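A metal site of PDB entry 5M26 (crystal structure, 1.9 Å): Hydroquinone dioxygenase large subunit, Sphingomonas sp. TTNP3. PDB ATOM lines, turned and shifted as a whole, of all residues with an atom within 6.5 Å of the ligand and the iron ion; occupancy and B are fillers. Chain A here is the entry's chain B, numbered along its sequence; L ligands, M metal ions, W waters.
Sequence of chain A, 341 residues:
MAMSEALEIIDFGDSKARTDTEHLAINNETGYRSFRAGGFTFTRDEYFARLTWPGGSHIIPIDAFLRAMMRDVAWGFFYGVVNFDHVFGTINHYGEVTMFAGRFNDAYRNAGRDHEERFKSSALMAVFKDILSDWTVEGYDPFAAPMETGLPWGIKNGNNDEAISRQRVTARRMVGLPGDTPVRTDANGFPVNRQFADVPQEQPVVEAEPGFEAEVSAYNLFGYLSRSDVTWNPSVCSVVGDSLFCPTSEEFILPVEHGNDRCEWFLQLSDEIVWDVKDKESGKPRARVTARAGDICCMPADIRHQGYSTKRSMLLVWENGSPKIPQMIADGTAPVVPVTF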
ATOM      1  N   TRP A  75     -16.780  12.318  16.004  1.00  0.00           N
ATOM      2  CA  TRP A  75     -17.899  11.461  15.570  1.00  0.00           C
ATOM      3  C   TRP A  75     -18.931  12.182  14.725  1.00  0.00           C
ATOM      4  O   TRP A  75     -19.933  11.579  14.313  1.00  0.00           O
ATOM      5  CB  TRP A  75     -18.605  10.868  16.795  1.00  0.00           C
ATOM      6  CG  TRP A  75     -17.745  10.063  17.690  1.00  0.00           C
ATOM      7  CD1 TRP A  75     -16.562   9.437  17.380  1.00  0.00           C
ATOM      8  CD2 TRP A  75     -18.012   9.755  19.064  1.00  0.00           C
ATOM      9  NE1 TRP A  75     -16.074   8.786  18.492  1.00  0.00           N
ATOM     10  CE2 TRP A  75     -16.937   8.961  19.535  1.00  0.00           C
ATOM     11  CE3 TRP A  75     -19.042  10.098  19.955  1.00  0.00           C
ATOM     12  CZ2 TRP A  75     -16.868   8.484  20.851  1.00  0.00           C
ATOM     13  CZ3 TRP A  75     -18.986   9.612  21.265  1.00  0.00           C
ATOM     14  CH2 TRP A  75     -17.881   8.814  21.692  1.00  0.00           C
ATOM     15  N   PHE A  78     -22.214  11.843  16.189  1.00  0.00           N
ATOM     16  CA  PHE A  78     -22.504  10.420  16.468  1.00  0.00           C
ATOM     17  C   PHE A  78     -23.966  10.059  16.175  1.00  0.00           C
ATOM     18  O   PHE A  78     -24.558  10.609  15.262  1.00  0.00           O
ATOM     19  CB  PHE A  78     -22.056  10.061  17.915  1.00  0.00           C
ATOM     20  CG  PHE A  78     -21.710   8.599  18.099  1.00  0.00           C
ATOM     21  CD1 PHE A  78     -21.209   7.844  17.040  1.00  0.00           C
ATOM     22  CD2 PHE A  78     -21.860   7.983  19.350  1.00  0.00           C
ATOM     23  CE1 PHE A  78     -20.902   6.495  17.197  1.00  0.00           C
ATOM     24  CE2 PHE A  78     -21.521   6.638  19.513  1.00  0.00           C
ATOM     25  CZ  PHE A  78     -21.050   5.885  18.436  1.00  0.00           C
ATOM     26  N   THR A 231      -8.428   6.569  21.784  1.00  0.00           N
ATOM     27  CA  THR A 231      -9.302   5.720  22.608  1.00  0.00           C
ATOM     28  C   THR A 231     -10.777   6.054  22.392  1.00  0.00           C
ATOM     29  O   THR A 231     -11.100   7.206  22.095  1.00  0.00           O
ATOM     30  CB  THR A 231      -8.958   5.856  24.097  1.00  0.00           C
ATOM     31  OG1 THR A 231      -9.050   7.236  24.484  1.00  0.00           O
ATOM     32  CG2 THR A 231      -7.524   5.383  24.326  1.00  0.00           C
ATOM     33  N   TRP A 232     -11.657   5.064  22.528  1.00  0.00           N
ATOM     34  CA  TRP A 232     -13.104   5.321  22.477  1.00  0.00           C
ATOM     35  C   TRP A 232     -13.477   6.038  21.168  1.00  0.00           C
ATOM     36  O   TRP A 232     -13.929   7.184  21.176  1.00  0.00           O
ATOM     37  CB  TRP A 232     -13.570   6.129  23.694  1.00  0.00           C
ATOM     38  CG  TRP A 232     -13.202   5.536  25.054  1.00  0.00           C
ATOM     39  CD1 TRP A 232     -12.251   6.014  25.924  1.00  0.00           C
ATOM     40  CD2 TRP A 232     -13.799   4.385  25.725  1.00  0.00           C
ATOM     41  NE1 TRP A 232     -12.229   5.236  27.067  1.00  0.00           N
ATOM     42  CE2 TRP A 232     -13.160   4.247  26.974  1.00  0.00           C
ATOM     43  CE3 TRP A 232     -14.827   3.487  25.393  1.00  0.00           C
ATOM     44  CZ2 TRP A 232     -13.490   3.226  27.890  1.00  0.00           C
ATOM     45  CZ3 TRP A 232     -15.167   2.469  26.309  1.00  0.00           C
ATOM     46  CH2 TRP A 232     -14.498   2.357  27.534  1.00  0.00           C
ATOM     47  N   ASN A 233     -13.236   5.352  20.058  1.00  0.00           N
ATOM     48  CA  ASN A 233     -13.472   5.901  18.743  1.00  0.00           C
ATOM     49  C   ASN A 233     -13.972   4.831  17.766  1.00  0.00           C
ATOM     50  O   ASN A 233     -13.236   4.379  16.914  1.00  0.00           O
ATOM     51  CB  ASN A 233     -12.219   6.591  18.196  1.00  0.00           C
ATOM     52  CG  ASN A 233     -12.521   7.514  17.007  1.00  0.00           C
ATOM     53  OD1 ASN A 233     -13.563   8.183  16.975  1.00  0.00           O
ATOM     54  ND2 ASN A 233     -11.640   7.507  16.007  1.00  0.00           N
ATOM     55  N   PRO A 234     -15.240   4.432  17.886  1.00  0.00           N
ATOM     56  CA  PRO A 234     -15.766   3.384  17.000  1.00  0.00           C
ATOM     57  C   PRO A 234     -15.486   3.767  15.543  1.00  0.00           C
ATOM     58  O   PRO A 234     -15.785   4.890  15.137  1.00  0.00           O
ATOM     59  CB  PRO A 234     -17.264   3.441  17.274  1.00  0.00           C
ATOM     60  CG  PRO A 234     -17.349   3.885  18.705  1.00  0.00           C
ATOM     61  CD  PRO A 234     -16.298   4.962  18.775  1.00  0.00           C
ATOM     62  N   THR A 248     -12.731  -0.553  18.131  1.00  0.00           N
ATOM     63  CA  THR A 248     -11.999   0.585  18.726  1.00  0.00           C
ATOM     64  C   THR A 248     -11.128   0.063  19.890  1.00  0.00           C
ATOM     65  O   THR A 248     -11.358  -1.047  20.379  1.00  0.00           O
ATOM     66  CB  THR A 248     -12.987   1.722  19.147  1.00  0.00           C
ATOM     67  OG1 THR A 248     -12.302   2.740  19.910  1.00  0.00           O
ATOM     68  CG2 THR A 248     -14.186   1.183  19.944  1.00  0.00           C
ATOM     69  N   SER A 249     -10.121   0.823  20.307  1.00  0.00           N
ATOM     70  CA  SER A 249      -9.362   0.455  21.489  1.00  0.00           C
ATOM     71  C   SER A 249      -9.757   1.361  22.641  1.00  0.00           C
ATOM     72  O   SER A 249      -9.731   2.564  22.482  1.00  0.00           O
ATOM     73  CB  SER A 249      -7.886   0.606  21.215  1.00  0.00           C
ATOM     74  OG  SER A 249      -7.635   1.929  20.742  1.00  0.00           O
ATOM     75  N   GLU A 250     -10.092   0.786  23.800  1.00  0.00           N
ATOM     76  CA  GLU A 250     -10.697   1.544  24.900  1.00  0.00           C
ATOM     77  C   GLU A 250      -9.785   1.478  26.115  1.00  0.00           C
ATOM     78  O   GLU A 250      -9.278   0.418  26.444  1.00  0.00           O
ATOM     79  CB  GLU A 250     -12.032   0.924  25.312  1.00  0.00           C
ATOM     80  CG  GLU A 250     -12.939   0.447  24.169  1.00  0.00           C
ATOM     81  CD  GLU A 250     -13.413   1.570  23.266  1.00  0.00           C
ATOM     82  OE1 GLU A 250     -12.576   2.373  22.828  1.00  0.00           O
ATOM     83  OE2 GLU A 250     -14.627   1.656  22.964  1.00  0.00           O
ATOM     84  N   LEU A 254     -15.127   6.019  28.965  1.00  0.00           N
ATOM     85  CA  LEU A 254     -15.774   6.625  27.790  1.00  0.00           C
ATOM     86  C   LEU A 254     -16.119   8.065  28.193  1.00  0.00           C
ATOM     87  O   LEU A 254     -16.760   8.250  29.231  1.00  0.00           O
ATOM     88  CB  LEU A 254     -17.041   5.866  27.432  1.00  0.00           C
ATOM     89  CG  LEU A 254     -17.851   6.489  26.289  1.00  0.00           C
ATOM     90  CD1 LEU A 254     -17.028   6.562  24.998  1.00  0.00           C
ATOM     91  CD2 LEU A 254     -19.104   5.642  26.112  1.00  0.00           C
ATOM     92  N   VAL A 256     -18.185  10.221  27.363  1.00  0.00           N
ATOM     93  CA  VAL A 256     -19.589  10.620  27.362  1.00  0.00           C
ATOM     94  C   VAL A 256     -20.509   9.507  27.913  1.00  0.00           C
ATOM     95  O   VAL A 256     -20.070   8.355  28.047  1.00  0.00           O
ATOM     96  CB  VAL A 256     -20.053  10.995  25.943  1.00  0.00           C
ATOM     97  CG1 VAL A 256     -19.140  12.084  25.326  1.00  0.00           C
ATOM     98  CG2 VAL A 256     -20.137   9.752  25.040  1.00  0.00           C
ATOM     99  N   HIS A 258     -23.563   7.701  26.339  1.00  0.00           N
ATOM    100  CA  HIS A 258     -24.205   7.656  25.051  1.00  0.00           C
ATOM    101  C   HIS A 258     -25.625   7.163  25.157  1.00  0.00           C
ATOM    102  O   HIS A 258     -25.848   6.041  25.596  1.00  0.00           O
ATOM    103  CB  HIS A 258     -23.456   6.754  24.118  1.00  0.00           C
ATOM    104  CG  HIS A 258     -24.060   6.695  22.767  1.00  0.00           C
ATOM    105  ND1 HIS A 258     -24.075   5.543  22.006  1.00  0.00           N
ATOM    106  CD2 HIS A 258     -24.646   7.653  22.013  1.00  0.00           C
ATOM    107  CE1 HIS A 258     -24.649   5.798  20.846  1.00  0.00           C
ATOM    108  NE2 HIS A 258     -25.011   7.071  20.820  1.00  0.00           N
ATOM    109  N   GLY A 259     -26.577   7.989  24.747  1.00  0.00           N
ATOM    110  CA  GLY A 259     -27.990   7.554  24.723  1.00  0.00           C
ATOM    111  C   GLY A 259     -28.363   7.391  23.258  1.00  0.00           C
ATOM    112  O   GLY A 259     -28.759   8.360  22.619  1.00  0.00           O
ATOM    113  N   ASN A 260     -28.229   6.186  22.726  1.00  0.00           N
ATOM    114  CA  ASN A 260     -28.445   5.991  21.299  1.00  0.00           C
ATOM    115  C   ASN A 260     -29.916   6.126  20.953  1.00  0.00           C
ATOM    116  O   ASN A 260     -30.777   5.951  21.825  1.00  0.00           O
ATOM    117  CB  ASN A 260     -27.917   4.638  20.835  1.00  0.00           C
ATOM    118  CG  ASN A 260     -27.455   4.650  19.400  1.00  0.00           C
ATOM    119  OD1 ASN A 260     -27.763   5.564  18.632  1.00  0.00           O
ATOM    120  ND2 ASN A 260     -26.691   3.635  19.032  1.00  0.00           N
ATOM    121  N   GLU A 264     -27.948  -0.841  19.899  1.00  0.00           N
ATOM    122  CA  GLU A 264     -26.586  -1.079  19.406  1.00  0.00           C
ATOM    123  C   GLU A 264     -25.962  -2.226  20.194  1.00  0.00           C
ATOM    124  O   GLU A 264     -26.418  -2.543  21.292  1.00  0.00           O
ATOM    125  CB  GLU A 264     -25.759   0.224  19.427  1.00  0.00           C
ATOM    126  CG  GLU A 264     -25.015   0.436  20.706  1.00  0.00           C
ATOM    127  CD  GLU A 264     -24.451   1.842  20.866  1.00  0.00           C
ATOM    128  OE1 GLU A 264     -24.562   2.711  19.967  1.00  0.00           O
ATOM    129  OE2 GLU A 264     -23.875   2.080  21.918  1.00  0.00           O
ATOM    130  N   PHE A 266     -22.417  -4.482  21.657  1.00  0.00           N
ATOM    131  CA  PHE A 266     -21.012  -4.520  22.029  1.00  0.00           C
ATOM    132  C   PHE A 266     -20.520  -5.950  22.068  1.00  0.00           C
ATOM    133  O   PHE A 266     -21.054  -6.782  22.828  1.00  0.00           O
ATOM    134  CB  PHE A 266     -20.845  -3.968  23.446  1.00  0.00           C
ATOM    135  CG  PHE A 266     -21.145  -2.520  23.594  1.00  0.00           C
ATOM    136  CD1 PHE A 266     -20.903  -1.624  22.552  1.00  0.00           C
ATOM    137  CD2 PHE A 266     -21.640  -2.021  24.801  1.00  0.00           C
ATOM    138  CE1 PHE A 266     -21.167  -0.267  22.698  1.00  0.00           C
ATOM    139  CE2 PHE A 266     -21.897  -0.672  24.960  1.00  0.00           C
ATOM    140  CZ  PHE A 266     -21.658   0.214  23.889  1.00  0.00           C
ATOM    141  N   TRP A 275     -19.799  -1.545  31.847  1.00  0.00           N
ATOM    142  CA  TRP A 275     -20.685  -0.502  31.328  1.00  0.00           C
ATOM    143  C   TRP A 275     -21.631  -0.081  32.449  1.00  0.00           C
ATOM    144  O   TRP A 275     -22.341  -0.910  33.056  1.00  0.00           O
ATOM    145  CB  TRP A 275     -21.506  -1.005  30.132  1.00  0.00           C
ATOM    146  CG  TRP A 275     -20.635  -1.396  28.975  1.00  0.00           C
ATOM    147  CD1 TRP A 275     -20.213  -2.650  28.646  1.00  0.00           C
ATOM    148  CD2 TRP A 275     -20.061  -0.507  27.997  1.00  0.00           C
ATOM    149  NE1 TRP A 275     -19.410  -2.603  27.527  1.00  0.00           N
ATOM    150  CE2 TRP A 275     -19.298  -1.291  27.115  1.00  0.00           C
ATOM    151  CE3 TRP A 275     -20.112   0.893  27.794  1.00  0.00           C
ATOM    152  CZ2 TRP A 275     -18.599  -0.752  26.028  1.00  0.00           C
ATOM    153  CZ3 TRP A 275     -19.399   1.444  26.691  1.00  0.00           C
ATOM    154  CH2 TRP A 275     -18.658   0.620  25.836  1.00  0.00           C
ATOM    155  N   MET A 299     -27.185  -2.853  23.983  1.00  0.00           N
ATOM    156  CA  MET A 299     -27.565  -1.700  24.731  1.00  0.00           C
ATOM    157  C   MET A 299     -28.959  -1.310  24.186  1.00  0.00           C
ATOM    158  O   MET A 299     -29.055  -0.887  23.021  1.00  0.00           O
ATOM    159  CB  MET A 299     -26.591  -0.538  24.510  1.00  0.00           C
ATOM    160  CG  MET A 299     -25.219  -0.644  25.189  1.00  0.00           C
ATOM    161  SD  MET A 299     -25.365  -0.749  26.989  1.00  0.00           S
ATOM    162  CE  MET A 299     -24.998  -2.487  27.198  1.00  0.00           C
ATOM    163  N   HIS A 305     -25.241   4.735  28.256  1.00  0.00           N
ATOM    164  CA  HIS A 305     -24.188   3.867  28.778  1.00  0.00           C
ATOM    165  C   HIS A 305     -22.860   4.578  28.784  1.00  0.00           C
ATOM    166  O   HIS A 305     -22.606   5.446  27.932  1.00  0.00           O
ATOM    167  CB  HIS A 305     -24.085   2.585  27.946  1.00  0.00           C
ATOM    168  CG  HIS A 305     -24.195   2.818  26.468  1.00  0.00           C
ATOM    169  ND1 HIS A 305     -25.395   2.838  25.814  1.00  0.00           N
ATOM    170  CD2 HIS A 305     -23.250   3.063  25.528  1.00  0.00           C
ATOM    171  CE1 HIS A 305     -25.200   3.082  24.535  1.00  0.00           C
ATOM    172  NE2 HIS A 305     -23.910   3.239  24.332  1.00  0.00           N
ATOM    173  N   LEU A 315     -12.670  -3.570  21.557  1.00  0.00           N
ATOM    174  CA  LEU A 315     -14.139  -3.667  21.607  1.00  0.00           C
ATOM    175  C   LEU A 315     -14.667  -3.541  20.190  1.00  0.00           C
ATOM    176  O   LEU A 315     -14.193  -2.701  19.433  1.00  0.00           O
ATOM    177  CB  LEU A 315     -14.703  -2.531  22.455  1.00  0.00           C
ATOM    178  CG  LEU A 315     -16.216  -2.319  22.406  1.00  0.00           C
ATOM    179  CD1 LEU A 315     -16.961  -3.439  23.156  1.00  0.00           C
ATOM    180  CD2 LEU A 315     -16.498  -0.945  22.998  1.00  0.00           C
ATOM    181  N   VAL A 317     -17.906  -2.332  18.355  1.00  0.00           N
ATOM    182  CA  VAL A 317     -19.201  -1.705  18.472  1.00  0.00           C
ATOM    183  C   VAL A 317     -19.918  -2.000  17.145  1.00  0.00           C
ATOM    184  O   VAL A 317     -19.381  -1.727  16.056  1.00  0.00           O
ATOM    185  CB  VAL A 317     -19.093  -0.183  18.722  1.00  0.00           C
ATOM    186  CG1 VAL A 317     -20.466   0.496  18.688  1.00  0.00           C
ATOM    187  CG2 VAL A 317     -18.431   0.071  20.070  1.00  0.00           C
ATOM    188  N   GLU A 319     -23.176  -1.288  14.810  1.00  0.00           N
ATOM    189  CA  GLU A 319     -24.276  -0.360  14.570  1.00  0.00           C
ATOM    190  C   GLU A 319     -25.107  -0.758  13.347  1.00  0.00           C
ATOM    191  O   GLU A 319     -24.593  -1.330  12.391  1.00  0.00           O
ATOM    192  CB  GLU A 319     -23.783   1.076  14.308  1.00  0.00           C
ATOM    193  CG  GLU A 319     -22.954   1.709  15.391  1.00  0.00           C
ATOM    194  CD  GLU A 319     -23.752   2.245  16.572  1.00  0.00           C
ATOM    195  OE1 GLU A 319     -23.073   2.614  17.554  1.00  0.00           O
ATOM    196  OE2 GLU A 319     -25.005   2.343  16.549  1.00  0.00           O
HETATM  197  O1  LIG L   1     -15.710   3.779  21.980  1.00  0.00           O
HETATM  198  C1  LIG L   1     -17.040   3.838  22.161  1.00  0.00           C
HETATM  199  C2  LIG L   1     -17.685   2.697  22.598  1.00  0.00           C
HETATM  200  C3  LIG L   1     -19.065   2.727  22.784  1.00  0.00           C
HETATM  201  C4  LIG L   1     -17.743   5.010  21.908  1.00  0.00           C
HETATM  202  C5  LIG L   1     -19.136   5.031  22.088  1.00  0.00           C
HETATM  203  C6  LIG L   1     -19.812   3.893  22.537  1.00  0.00           C
HETATM  204  O2  LIG L   1     -21.169   3.894  22.721  1.00  0.00           O
HETATM  205  C7  LIG L   1     -19.897   6.287  21.831  1.00  0.00           C
HETATM  206 FE    FE M   1     -23.081   3.706  22.465  1.00  0.00          FE
HETATM  207  O   HOH W   1     -22.119   3.562  20.211  1.00  0.00           O
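The side-chain carboxylate (OE2) of Glu 250 is in hydrogen-bond range of an oxygen (O1) of the ligand (2.6 Å).
The iron ion is bound by OE2 of Glu 264 (1.9 Å), O2 of the ligand (1.9 Å), NE2 of His 305 (2.1 Å), ND1 of His 258 (2.1 Å) and water W1 (2.5 Å). The iron ion has five donor atoms within binding distance.
Water W1 bridges OE1 of Glu 264 and OE1 of Glu 319.
Trp 75 touches the ligand (CH2 to C7, 3.2 Å). CE2 of Phe 78 touches C7 of the ligand (2.9 Å). Trp 232 touches the ligand (CA to O1, 3.1 Å). Asn 233 touches the ligand. CG of Pro 234 touches C4 of the ligand, at 3.4 Å. CG2 of Thr 248 touches O1 of the ligand, 3.6 Å away. Leu 254 touches the ligand (CD1 to C4, 3.5 Å). CE1 of Phe 266 touches C3 of the ligand, at 3.7 Å. Trp 275 touches the ligand. Leu 315 touches the ligand (CD2 to C2, 3.9 Å). Val 317 touches the ligand. 15 residues have an atom within 4 Å of the ligand: Trp 75, Phe 78, Trp 232, Asn 233, Pro 234, Thr 248, Glu 250, Leu 254, His 258, Glu 264, Phe 266, Trp 275, His 305, Leu 315 and Val 317. Along chain A the residues within 4 Å of the ligand span positions 75 to 317.
ND2 of Asn 260 lies within hydrogen-bond range of OE1 of Glu 264 (2.5 Å). ND1 of His 305 sits close to SD of Met 299, 3.8 Å away. The backbone NH (N) of Trp 232 lies within hydrogen-bond range of the side-chain carboxylate (OE1) of Glu 250 (2.9 Å). The side-chain hydroxyl (OG1) of Thr 248 is in hydrogen-bond range of the side-chain carboxylate (OE1) of Glu 250, 3.0 Å away. N of Trp 232 lies within hydrogen-bond range of O of Ser 249, 3.2 Å away. OD1 of Asn 233 sits at hydrogen-bond distance from NE1 of Trp 75. N of Asn 233 is in hydrogen-bond range of OG1 of Thr 248, 2.8 Å away. The backbone carbonyl oxygen of Leu 315 lies within hydrogen-bond range of the backbone NH of Thr 248 (2.9 Å).
Within 4 Å of the iron ion: His 258, Glu 264 and His 305.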
